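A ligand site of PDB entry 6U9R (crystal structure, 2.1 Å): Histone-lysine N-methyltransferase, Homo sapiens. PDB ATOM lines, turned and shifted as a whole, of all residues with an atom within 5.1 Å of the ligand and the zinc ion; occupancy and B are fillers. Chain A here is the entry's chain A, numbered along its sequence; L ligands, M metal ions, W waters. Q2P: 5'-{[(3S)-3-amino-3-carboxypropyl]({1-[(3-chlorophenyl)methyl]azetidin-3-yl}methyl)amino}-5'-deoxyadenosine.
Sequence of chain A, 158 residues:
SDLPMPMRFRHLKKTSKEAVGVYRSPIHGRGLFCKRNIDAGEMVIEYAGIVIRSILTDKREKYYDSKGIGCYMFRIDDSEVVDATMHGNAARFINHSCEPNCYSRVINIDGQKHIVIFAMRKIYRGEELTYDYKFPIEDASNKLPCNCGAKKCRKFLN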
ATOM      1  N   ILE A  27      21.925 -13.501  11.595  1.00  0.00           N
ATOM      2  CA  ILE A  27      20.931 -12.997  10.658  1.00  0.00           C
ATOM      3  C   ILE A  27      20.183 -11.869  11.375  1.00  0.00           C
ATOM      4  O   ILE A  27      20.211 -10.745  10.898  1.00  0.00           O
ATOM      5  CB  ILE A  27      19.990 -14.118  10.081  1.00  0.00           C
ATOM      6  CG1 ILE A  27      20.754 -15.040   9.125  1.00  0.00           C
ATOM      7  CG2 ILE A  27      18.780 -13.514   9.387  1.00  0.00           C
ATOM      8  CD1 ILE A  27      20.050 -16.442   8.857  1.00  0.00           C
ATOM      9  N   HIS A  28      19.582 -12.161  12.549  1.00  0.00           N
ATOM     10  CA  HIS A  28      18.856 -11.192  13.383  1.00  0.00           C
ATOM     11  C   HIS A  28      18.546 -11.800  14.748  1.00  0.00           C
ATOM     12  O   HIS A  28      18.065 -12.943  14.812  1.00  0.00           O
ATOM     13  CB  HIS A  28      17.528 -10.789  12.705  1.00  0.00           C
ATOM     14  CG  HIS A  28      16.646  -9.887  13.521  1.00  0.00           C
ATOM     15  ND1 HIS A  28      15.882 -10.379  14.592  1.00  0.00           N
ATOM     16  CD2 HIS A  28      16.392  -8.566  13.387  1.00  0.00           C
ATOM     17  CE1 HIS A  28      15.222  -9.345  15.068  1.00  0.00           C
ATOM     18  NE2 HIS A  28      15.459  -8.231  14.354  1.00  0.00           N
ATOM     19  N   GLY A  29      18.714 -10.978  15.792  1.00  0.00           N
ATOM     20  CA  GLY A  29      18.379 -11.280  17.189  1.00  0.00           C
ATOM     21  C   GLY A  29      18.684 -12.688  17.609  1.00  0.00           C
ATOM     22  O   GLY A  29      19.854 -13.080  17.664  1.00  0.00           O
ATOM     23  N   ARG A  30      17.636 -13.472  17.893  1.00  0.00           N
ATOM     24  CA  ARG A  30      17.821 -14.883  18.224  1.00  0.00           C
ATOM     25  C   ARG A  30      17.253 -15.712  17.106  1.00  0.00           C
ATOM     26  O   ARG A  30      16.333 -15.274  16.414  1.00  0.00           O
ATOM     27  CB  ARG A  30      17.186 -15.253  19.590  1.00  0.00           C
ATOM     28  CG  ARG A  30      17.997 -14.764  20.805  1.00  0.00           C
ATOM     29  CD  ARG A  30      17.248 -14.985  22.108  1.00  0.00           C
ATOM     30  NE  ARG A  30      15.996 -14.210  22.139  1.00  0.00           N
ATOM     31  CZ  ARG A  30      15.049 -14.332  23.059  1.00  0.00           C
ATOM     32  NH1 ARG A  30      15.167 -15.229  24.038  1.00  0.00           N
ATOM     33  NH2 ARG A  30      13.969 -13.564  23.021  1.00  0.00           N
ATOM     34  N   GLY A  31      17.818 -16.885  16.893  1.00  0.00           N
ATOM     35  CA  GLY A  31      17.331 -17.794  15.871  1.00  0.00           C
ATOM     36  C   GLY A  31      17.201 -19.218  16.394  1.00  0.00           C
ATOM     37  O   GLY A  31      17.640 -19.513  17.521  1.00  0.00           O
ATOM     38  N   GLY A  70       7.430  -8.489  22.816  1.00  0.00           N
ATOM     39  CA  GLY A  70       7.671  -8.844  21.430  1.00  0.00           C
ATOM     40  C   GLY A  70       6.469  -9.565  20.874  1.00  0.00           C
ATOM     41  O   GLY A  70       5.870 -10.405  21.552  1.00  0.00           O
ATOM     42  N   CYS A  71       6.036  -9.187  19.676  1.00  0.00           N
ATOM     43  CA  CYS A  71       4.869  -9.751  18.993  1.00  0.00           C
ATOM     44  C   CYS A  71       5.355 -10.807  18.030  1.00  0.00           C
ATOM     45  O   CYS A  71       6.128 -10.480  17.148  1.00  0.00           O
ATOM     46  CB  CYS A  71       4.096  -8.660  18.267  1.00  0.00           C
ATOM     47  SG  CYS A  71       2.626  -9.261  17.410  1.00  0.00           S
ATOM     48  N   TYR A  72       4.939 -12.062  18.176  1.00  0.00           N
ATOM     49  CA  TYR A  72       5.379 -13.186  17.332  1.00  0.00           C
ATOM     50  C   TYR A  72       4.135 -13.742  16.636  1.00  0.00           C
ATOM     51  O   TYR A  72       3.299 -14.365  17.267  1.00  0.00           O
ATOM     52  CB  TYR A  72       6.048 -14.288  18.205  1.00  0.00           C
ATOM     53  CG  TYR A  72       7.394 -13.876  18.758  1.00  0.00           C
ATOM     54  CD1 TYR A  72       8.570 -14.175  18.076  1.00  0.00           C
ATOM     55  CD2 TYR A  72       7.499 -13.174  19.956  1.00  0.00           C
ATOM     56  CE1 TYR A  72       9.812 -13.772  18.552  1.00  0.00           C
ATOM     57  CE2 TYR A  72       8.750 -12.737  20.440  1.00  0.00           C
ATOM     58  CZ  TYR A  72       9.896 -13.040  19.723  1.00  0.00           C
ATOM     59  OH  TYR A  72      11.155 -12.637  20.118  1.00  0.00           O
ATOM     60  N   ARG A  92       8.936 -19.846  17.075  1.00  0.00           N
ATOM     61  CA  ARG A  92       8.669 -18.424  16.850  1.00  0.00           C
ATOM     62  C   ARG A  92       9.958 -17.620  16.562  1.00  0.00           C
ATOM     63  O   ARG A  92       9.875 -16.490  16.082  1.00  0.00           O
ATOM     64  CB  ARG A  92       7.819 -17.803  17.996  1.00  0.00           C
ATOM     65  CG  ARG A  92       8.557 -17.585  19.289  1.00  0.00           C
ATOM     66  CD  ARG A  92       7.563 -17.237  20.408  1.00  0.00           C
ATOM     67  NE  ARG A  92       8.264 -16.779  21.617  1.00  0.00           N
ATOM     68  CZ  ARG A  92       8.694 -17.566  22.596  1.00  0.00           C
ATOM     69  NH1 ARG A  92       8.531 -18.875  22.526  1.00  0.00           N
ATOM     70  NH2 ARG A  92       9.312 -17.046  23.644  1.00  0.00           N
ATOM     71  N   PHE A  93      11.145 -18.205  16.850  1.00  0.00           N
ATOM     72  CA  PHE A  93      12.425 -17.548  16.582  1.00  0.00           C
ATOM     73  C   PHE A  93      13.031 -17.872  15.203  1.00  0.00           C
ATOM     74  O   PHE A  93      14.119 -17.370  14.917  1.00  0.00           O
ATOM     75  CB  PHE A  93      13.421 -17.854  17.690  1.00  0.00           C
ATOM     76  CG  PHE A  93      13.002 -17.339  19.040  1.00  0.00           C
ATOM     77  CD1 PHE A  93      13.184 -16.005  19.377  1.00  0.00           C
ATOM     78  CD2 PHE A  93      12.401 -18.187  19.958  1.00  0.00           C
ATOM     79  CE1 PHE A  93      12.797 -15.526  20.638  1.00  0.00           C
ATOM     80  CE2 PHE A  93      12.023 -17.711  21.225  1.00  0.00           C
ATOM     81  CZ  PHE A  93      12.232 -16.385  21.554  1.00  0.00           C
ATOM     82  N   ILE A  94      12.361 -18.687  14.355  1.00  0.00           N
ATOM     83  CA  ILE A  94      12.902 -19.049  13.031  1.00  0.00           C
ATOM     84  C   ILE A  94      13.005 -17.819  12.151  1.00  0.00           C
ATOM     85  O   ILE A  94      11.981 -17.201  11.829  1.00  0.00           O
ATOM     86  CB  ILE A  94      12.095 -20.185  12.324  1.00  0.00           C
ATOM     87  CG1 ILE A  94      12.043 -21.469  13.171  1.00  0.00           C
ATOM     88  CG2 ILE A  94      12.682 -20.497  10.904  1.00  0.00           C
ATOM     89  CD1 ILE A  94      11.009 -22.429  12.732  1.00  0.00           C
ATOM     90  N   ASN A  95      14.227 -17.468  11.728  1.00  0.00           N
ATOM     91  CA  ASN A  95      14.468 -16.327  10.837  1.00  0.00           C
ATOM     92  C   ASN A  95      14.188 -16.637   9.380  1.00  0.00           C
ATOM     93  O   ASN A  95      14.060 -17.795   9.012  1.00  0.00           O
ATOM     94  CB  ASN A  95      15.911 -15.800  10.980  1.00  0.00           C
ATOM     95  CG  ASN A  95      16.110 -14.993  12.233  1.00  0.00           C
ATOM     96  OD1 ASN A  95      15.268 -14.184  12.637  1.00  0.00           O
ATOM     97  ND2 ASN A  95      17.227 -15.199  12.888  1.00  0.00           N
ATOM     98  N   HIS A  96      14.080 -15.589   8.551  1.00  0.00           N
ATOM     99  CA  HIS A  96      13.886 -15.668   7.107  1.00  0.00           C
ATOM    100  C   HIS A  96      15.217 -15.899   6.367  1.00  0.00           C
ATOM    101  O   HIS A  96      16.264 -15.449   6.839  1.00  0.00           O
ATOM    102  CB  HIS A  96      13.259 -14.341   6.604  1.00  0.00           C
ATOM    103  CG  HIS A  96      13.271 -14.209   5.114  1.00  0.00           C
ATOM    104  ND1 HIS A  96      12.403 -14.921   4.317  1.00  0.00           N
ATOM    105  CD2 HIS A  96      14.091 -13.480   4.327  1.00  0.00           C
ATOM    106  CE1 HIS A  96      12.720 -14.597   3.072  1.00  0.00           C
ATOM    107  NE2 HIS A  96      13.742 -13.744   3.035  1.00  0.00           N
ATOM    108  N   SER A  97      15.157 -16.572   5.196  1.00  0.00           N
ATOM    109  CA  SER A  97      16.300 -16.763   4.287  1.00  0.00           C
ATOM    110  C   SER A  97      15.826 -16.976   2.872  1.00  0.00           C
ATOM    111  O   SER A  97      14.802 -17.611   2.668  1.00  0.00           O
ATOM    112  CB  SER A  97      17.193 -17.923   4.722  1.00  0.00           C
ATOM    113  OG  SER A  97      18.225 -18.189   3.783  1.00  0.00           O
ATOM    114  N   CYS A  98      16.618 -16.493   1.906  1.00  0.00           N
ATOM    115  CA  CYS A  98      16.345 -16.571   0.464  1.00  0.00           C
ATOM    116  C   CYS A  98      16.866 -17.876  -0.138  1.00  0.00           C
ATOM    117  O   CYS A  98      16.578 -18.186  -1.301  1.00  0.00           O
ATOM    118  CB  CYS A  98      16.884 -15.339  -0.249  1.00  0.00           C
ATOM    119  SG  CYS A  98      16.391 -13.789   0.532  1.00  0.00           S
ATOM    120  N   TYR A 133       9.954 -16.369   4.222  1.00  0.00           N
ATOM    121  CA  TYR A 133       8.747 -15.716   4.768  1.00  0.00           C
ATOM    122  C   TYR A 133       7.806 -15.395   3.625  1.00  0.00           C
ATOM    123  O   TYR A 133       8.279 -15.072   2.526  1.00  0.00           O
ATOM    124  CB  TYR A 133       9.116 -14.392   5.480  1.00  0.00           C
ATOM    125  CG  TYR A 133       9.651 -14.533   6.894  1.00  0.00           C
ATOM    126  CD1 TYR A 133      10.134 -15.755   7.370  1.00  0.00           C
ATOM    127  CD2 TYR A 133       9.726 -13.424   7.740  1.00  0.00           C
ATOM    128  CE1 TYR A 133      10.668 -15.864   8.654  1.00  0.00           C
ATOM    129  CE2 TYR A 133      10.266 -13.526   9.022  1.00  0.00           C
ATOM    130  CZ  TYR A 133      10.740 -14.750   9.471  1.00  0.00           C
ATOM    131  OH  TYR A 133      11.233 -14.863  10.738  1.00  0.00           O
ATOM    132  N   PHE A 135       5.979 -12.825   2.888  1.00  0.00           N
ATOM    133  CA  PHE A 135       6.191 -11.461   2.376  1.00  0.00           C
ATOM    134  C   PHE A 135       7.643 -11.256   1.942  1.00  0.00           C
ATOM    135  O   PHE A 135       7.918 -10.486   1.025  1.00  0.00           O
ATOM    136  CB  PHE A 135       5.775 -10.410   3.423  1.00  0.00           C
ATOM    137  CG  PHE A 135       6.562 -10.396   4.709  1.00  0.00           C
ATOM    138  CD1 PHE A 135       6.289 -11.321   5.719  1.00  0.00           C
ATOM    139  CD2 PHE A 135       7.542  -9.443   4.942  1.00  0.00           C
ATOM    140  CE1 PHE A 135       7.011 -11.307   6.913  1.00  0.00           C
ATOM    141  CE2 PHE A 135       8.249  -9.417   6.147  1.00  0.00           C
ATOM    142  CZ  PHE A 135       7.984 -10.345   7.125  1.00  0.00           C
ATOM    143  N   PRO A 145      14.974  -4.737   4.814  1.00  0.00           N
ATOM    144  CA  PRO A 145      16.180  -5.427   4.303  1.00  0.00           C
ATOM    145  C   PRO A 145      16.425  -6.817   4.859  1.00  0.00           C
ATOM    146  O   PRO A 145      16.077  -7.091   6.010  1.00  0.00           O
ATOM    147  CB  PRO A 145      17.326  -4.461   4.638  1.00  0.00           C
ATOM    148  CG  PRO A 145      16.822  -3.655   5.778  1.00  0.00           C
ATOM    149  CD  PRO A 145      15.329  -3.562   5.645  1.00  0.00           C
ATOM    150  N   CYS A 146      17.020  -7.713   4.036  1.00  0.00           N
ATOM    151  CA  CYS A 146      17.311  -9.096   4.397  1.00  0.00           C
ATOM    152  C   CYS A 146      18.801  -9.358   4.641  1.00  0.00           C
ATOM    153  O   CYS A 146      19.648  -8.959   3.824  1.00  0.00           O
ATOM    154  CB  CYS A 146      16.728 -10.049   3.359  1.00  0.00           C
ATOM    155  SG  CYS A 146      17.354 -11.739   3.478  1.00  0.00           S
ATOM    156  N   ASN A 147      19.100 -10.073   5.743  1.00  0.00           N
ATOM    157  CA  ASN A 147      20.449 -10.404   6.189  1.00  0.00           C
ATOM    158  C   ASN A 147      20.776 -11.912   6.143  1.00  0.00           C
ATOM    159  O   ASN A 147      21.728 -12.356   6.804  1.00  0.00           O
ATOM    160  CB  ASN A 147      20.683  -9.813   7.598  1.00  0.00           C
ATOM    161  CG  ASN A 147      22.131  -9.627   7.982  1.00  0.00           C
ATOM    162  OD1 ASN A 147      22.938  -9.046   7.238  1.00  0.00           O
ATOM    163  ND2 ASN A 147      22.507 -10.101   9.150  1.00  0.00           N
ATOM    164  N   CYS A 148      20.034 -12.705   5.338  1.00  0.00           N
ATOM    165  CA  CYS A 148      20.287 -14.150   5.271  1.00  0.00           C
ATOM    166  C   CYS A 148      21.724 -14.484   4.838  1.00  0.00           C
ATOM    167  O   CYS A 148      22.268 -15.501   5.270  1.00  0.00           O
ATOM    168  CB  CYS A 148      19.267 -14.865   4.396  1.00  0.00           C
ATOM    169  SG  CYS A 148      19.530 -14.664   2.616  1.00  0.00           S
ATOM    170  N   GLY A 149      22.272 -13.625   3.965  1.00  0.00           N
ATOM    171  CA  GLY A 149      23.636 -13.683   3.448  1.00  0.00           C
ATOM    172  C   GLY A 149      23.865 -14.621   2.276  1.00  0.00           C
ATOM    173  O   GLY A 149      25.010 -14.747   1.852  1.00  0.00           O
ATOM    174  N   CYS A 153      20.482 -13.859  -2.771  1.00  0.00           N
ATOM    175  CA  CYS A 153      19.635 -13.112  -1.835  1.00  0.00           C
ATOM    176  C   CYS A 153      18.686 -12.158  -2.571  1.00  0.00           C
ATOM    177  O   CYS A 153      19.130 -11.414  -3.435  1.00  0.00           O
ATOM    178  CB  CYS A 153      20.489 -12.369  -0.813  1.00  0.00           C
ATOM    179  SG  CYS A 153      19.534 -11.517   0.473  1.00  0.00           S
ATOM    180  N   ARG A 154      17.382 -12.156  -2.194  1.00  0.00           N
ATOM    181  CA  ARG A 154      16.351 -11.260  -2.770  1.00  0.00           C
ATOM    182  C   ARG A 154      16.539  -9.832  -2.237  1.00  0.00           C
ATOM    183  O   ARG A 154      15.928  -8.896  -2.750  1.00  0.00           O
ATOM    184  CB  ARG A 154      14.932 -11.773  -2.475  1.00  0.00           C
ATOM    185  N   LYS A 155      17.404  -9.686  -1.193  1.00  0.00           N
ATOM    186  CA  LYS A 155      17.870  -8.479  -0.505  1.00  0.00           C
ATOM    187  C   LYS A 155      16.796  -7.746   0.325  1.00  0.00           C
ATOM    188  O   LYS A 155      17.130  -6.814   1.080  1.00  0.00           O
ATOM    189  CB  LYS A 155      18.582  -7.531  -1.471  1.00  0.00           C
ATOM    190  CG  LYS A 155      19.767  -8.197  -2.217  1.00  0.00           C
ATOM    191  CD  LYS A 155      21.002  -8.439  -1.327  1.00  0.00           C
ATOM    192  CE  LYS A 155      22.196  -8.928  -2.113  1.00  0.00           C
ATOM    193  NZ  LYS A 155      23.382  -9.133  -1.242  1.00  0.00           N
HETATM  194  C1  Q2P L   1      16.645  -9.390   8.490  1.00  0.00           C
HETATM  195  O1  Q2P L   1      10.039  -9.536  11.065  1.00  0.00           O
HETATM  196  O2  Q2P L   1      15.004 -12.548  17.770  1.00  0.00           O
HETATM  197  C2  Q2P L   1      15.175 -10.661   9.683  1.00  0.00           C
HETATM  198  N   Q2P L   1      16.604 -12.613   6.919  1.00  0.00           N
HETATM  199  C3  Q2P L   1      15.406 -11.786   8.846  1.00  0.00           C
HETATM  200  O3  Q2P L   1      12.824 -12.485  17.971  1.00  0.00           O
HETATM  201  C4  Q2P L   1      13.999 -12.489  10.340  1.00  0.00           C
HETATM  202  C5  Q2P L   1      13.585 -10.229  11.594  1.00  0.00           C
HETATM  203  C6  Q2P L   1      12.452  -9.397  10.885  1.00  0.00           C
HETATM  204  C7  Q2P L   1      11.223 -10.263  11.088  1.00  0.00           C
HETATM  205  C8  Q2P L   1      11.557 -10.842  12.498  1.00  0.00           C
HETATM  206  C9  Q2P L   1      10.877 -12.208  12.741  1.00  0.00           C
HETATM  207  C10 Q2P L   1      10.114 -12.590  15.090  1.00  0.00           C
HETATM  208  C11 Q2P L   1       9.835 -11.088  15.323  1.00  0.00           C
HETATM  209  C12 Q2P L   1       8.986 -10.697  16.555  1.00  0.00           C
HETATM  210  C13 Q2P L   1      10.488  -9.532  18.337  1.00  0.00           C
HETATM  211  C14 Q2P L   1      11.681  -8.594  18.250  1.00  0.00           C
HETATM  212  C15 Q2P L   1      12.977  -9.062  18.542  1.00  0.00           C
HETATM  213  C16 Q2P L   1      14.066  -8.170  18.374  1.00  0.00           C
HETATM  214  C17 Q2P L   1      13.927  -6.851  17.957  1.00  0.00           C
HETATM  215  C18 Q2P L   1      12.619  -6.382  17.683  1.00  0.00           C
HETATM  216  C24 Q2P L   1      13.787 -12.630  17.241  1.00  0.00           C
HETATM  217  C23 Q2P L   1      13.766 -12.876  15.724  1.00  0.00           C
HETATM  218  N7  Q2P L   1      15.110 -13.165  15.173  1.00  0.00           N
HETATM  219  C22 Q2P L   1      12.852 -14.106  15.473  1.00  0.00           C
HETATM  220  C21 Q2P L   1      12.054 -13.970  14.143  1.00  0.00           C
HETATM  221  N5  Q2P L   1      11.241 -12.676  14.137  1.00  0.00           N
HETATM  222  O   Q2P L   1      12.310  -8.261  11.656  1.00  0.00           O
HETATM  223  O4  Q2P L   1      12.969 -11.034  12.542  1.00  0.00           O
HETATM  224  N4  Q2P L   1      14.244 -11.112  10.630  1.00  0.00           N
HETATM  225  N2  Q2P L   1      15.792  -9.414   9.556  1.00  0.00           N
HETATM  226  N1  Q2P L   1      16.940 -10.391   7.596  1.00  0.00           N
HETATM  227  N3  Q2P L   1      14.679 -12.917   9.278  1.00  0.00           N
HETATM  228  C   Q2P L   1      16.319 -11.595   7.771  1.00  0.00           C
HETATM  229  C20 Q2P L   1      11.008 -10.299  15.999  1.00  0.00           C
HETATM  230  N6  Q2P L   1      10.039  -9.674  16.928  1.00  0.00           N
HETATM  231  C19 Q2P L   1      11.491  -7.258  17.824  1.00  0.00           C
HETATM  232 CL   Q2P L   1      15.643  -8.734  18.760  1.00  0.00          CL
HETATM  233 ZN    ZN M   1      18.128 -13.087   1.808  1.00  0.00          ZN
HETATM  234  O   HOH W   1      14.289  -5.536  14.879  1.00  0.00           O
HETATM  235  O   HOH W   2       9.135  -7.398  14.872  1.00  0.00           O
HETATM  236  O   HOH W   3      15.402 -12.012  20.291  1.00  0.00           O
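Ile 27 touches the ligand (CG2 to N, 3.4 Å).
Gly 29 touches the ligand.
Cys 71 touches the ligand.
O of Arg 92 touches C21 of the ligand, at 3.9 Å.
Phe 93 touches the ligand.
Ile 94 touches the ligand (O to C21, 3.97 Å).
OH of Tyr 133 touches C9 of the ligand, at 3.3 Å.
Pro 145 touches the ligand (O to C1, 3.4 Å).
Hydrophobic or aromatic side chains within 4 Å of the ligand: Ile 27, His 28, Tyr 72, Phe 93, His 96 and Tyr 133.
Of the 25 residues printed, 16 come within 4 Å of the ligand.
The nearest printed residue that does not touch the ligand is Gly 70 (4.2 Å).
Water W3 lies within hydrogen-bond range of O2 of the ligand (2.6 Å) and NE of Arg 30 (2.9 Å).
A ring nitrogen (NE2) of His 96 lies close to the side-chain sulfur of Cys 98 (3.6 Å).
The backbone NH (N) of Arg 154 lies close to the side-chain sulfur (SG) of Cys 98 (3.3 Å).
The backbone carbonyl oxygen (O) of Lys 155 lies within hydrogen-bond range of the backbone NH (N) of Cys 146, 3.1 Å away.
N of Lys 155 lies close to SG of Cys 153 (3.3 Å).
The side-chain amide nitrogen of Asn 95 sits at hydrogen-bond distance from the backbone carbonyl oxygen of His 28 (3.1 Å).
A ring nitrogen (ND1) of His 96 is in hydrogen-bond range of the backbone NH of Tyr 133 (2.8 Å).
The backbone carbonyl oxygen (O) of Ile 27 sits at hydrogen-bond distance from the side-chain amide nitrogen (ND2) of Asn 147 (3.0 Å).
The backbone carbonyl oxygen (O) of Ile 94 lies within hydrogen-bond range of the side-chain hydroxyl (OH) of Tyr 133, at 2.7 Å.
SG of Cys 146 lies close to N of the ligand (3.6 Å).
The side-chain hydroxyl (OH) of Tyr 72 is in hydrogen-bond range of an oxygen (O3) of the ligand.
The backbone NH of Arg 30 is in hydrogen-bond range of an oxygen (O2) of the ligand (2.8 Å).
O of Arg 30 sits at hydrogen-bond distance from N7 of the ligand, at 2.7 Å.
A nitrogen (N7) of the ligand sits at hydrogen-bond distance from the side-chain amide oxygen of Asn 95.
A nitrogen (N3) of the ligand is in hydrogen-bond range of the backbone NH (N) of His 96 (2.8 Å).
A nitrogen (N) of the ligand is in hydrogen-bond range of the backbone carbonyl oxygen of His 96 (2.9 Å).
The backbone NH of Asn 147 sits at hydrogen-bond distance from a nitrogen (N1) of the ligand, at 2.9 Å.
The backbone carbonyl oxygen (O) of His 28 sits at hydrogen-bond distance from a nitrogen (N7) of the ligand.
N7 of the ligand lies within hydrogen-bond range of ND1 of His 28 (2.9 Å).
Within 4 Å of the zinc ion: Cys 98, Cys 146, Cys 148 and Cys 153.
The nearest printed residue that does not touch the zinc ion is Arg 154 (4.2 Å).
The zinc ion is bound by the side-chain sulfur (SG) of Cys 148 (2.3 Å), the side-chain sulfur (SG) of Cys 98 (2.3 Å), the side-chain sulfur (SG) of Cys 146 (2.3 Å) and the side-chain sulfur (SG) of Cys 153 (2.5 Å).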
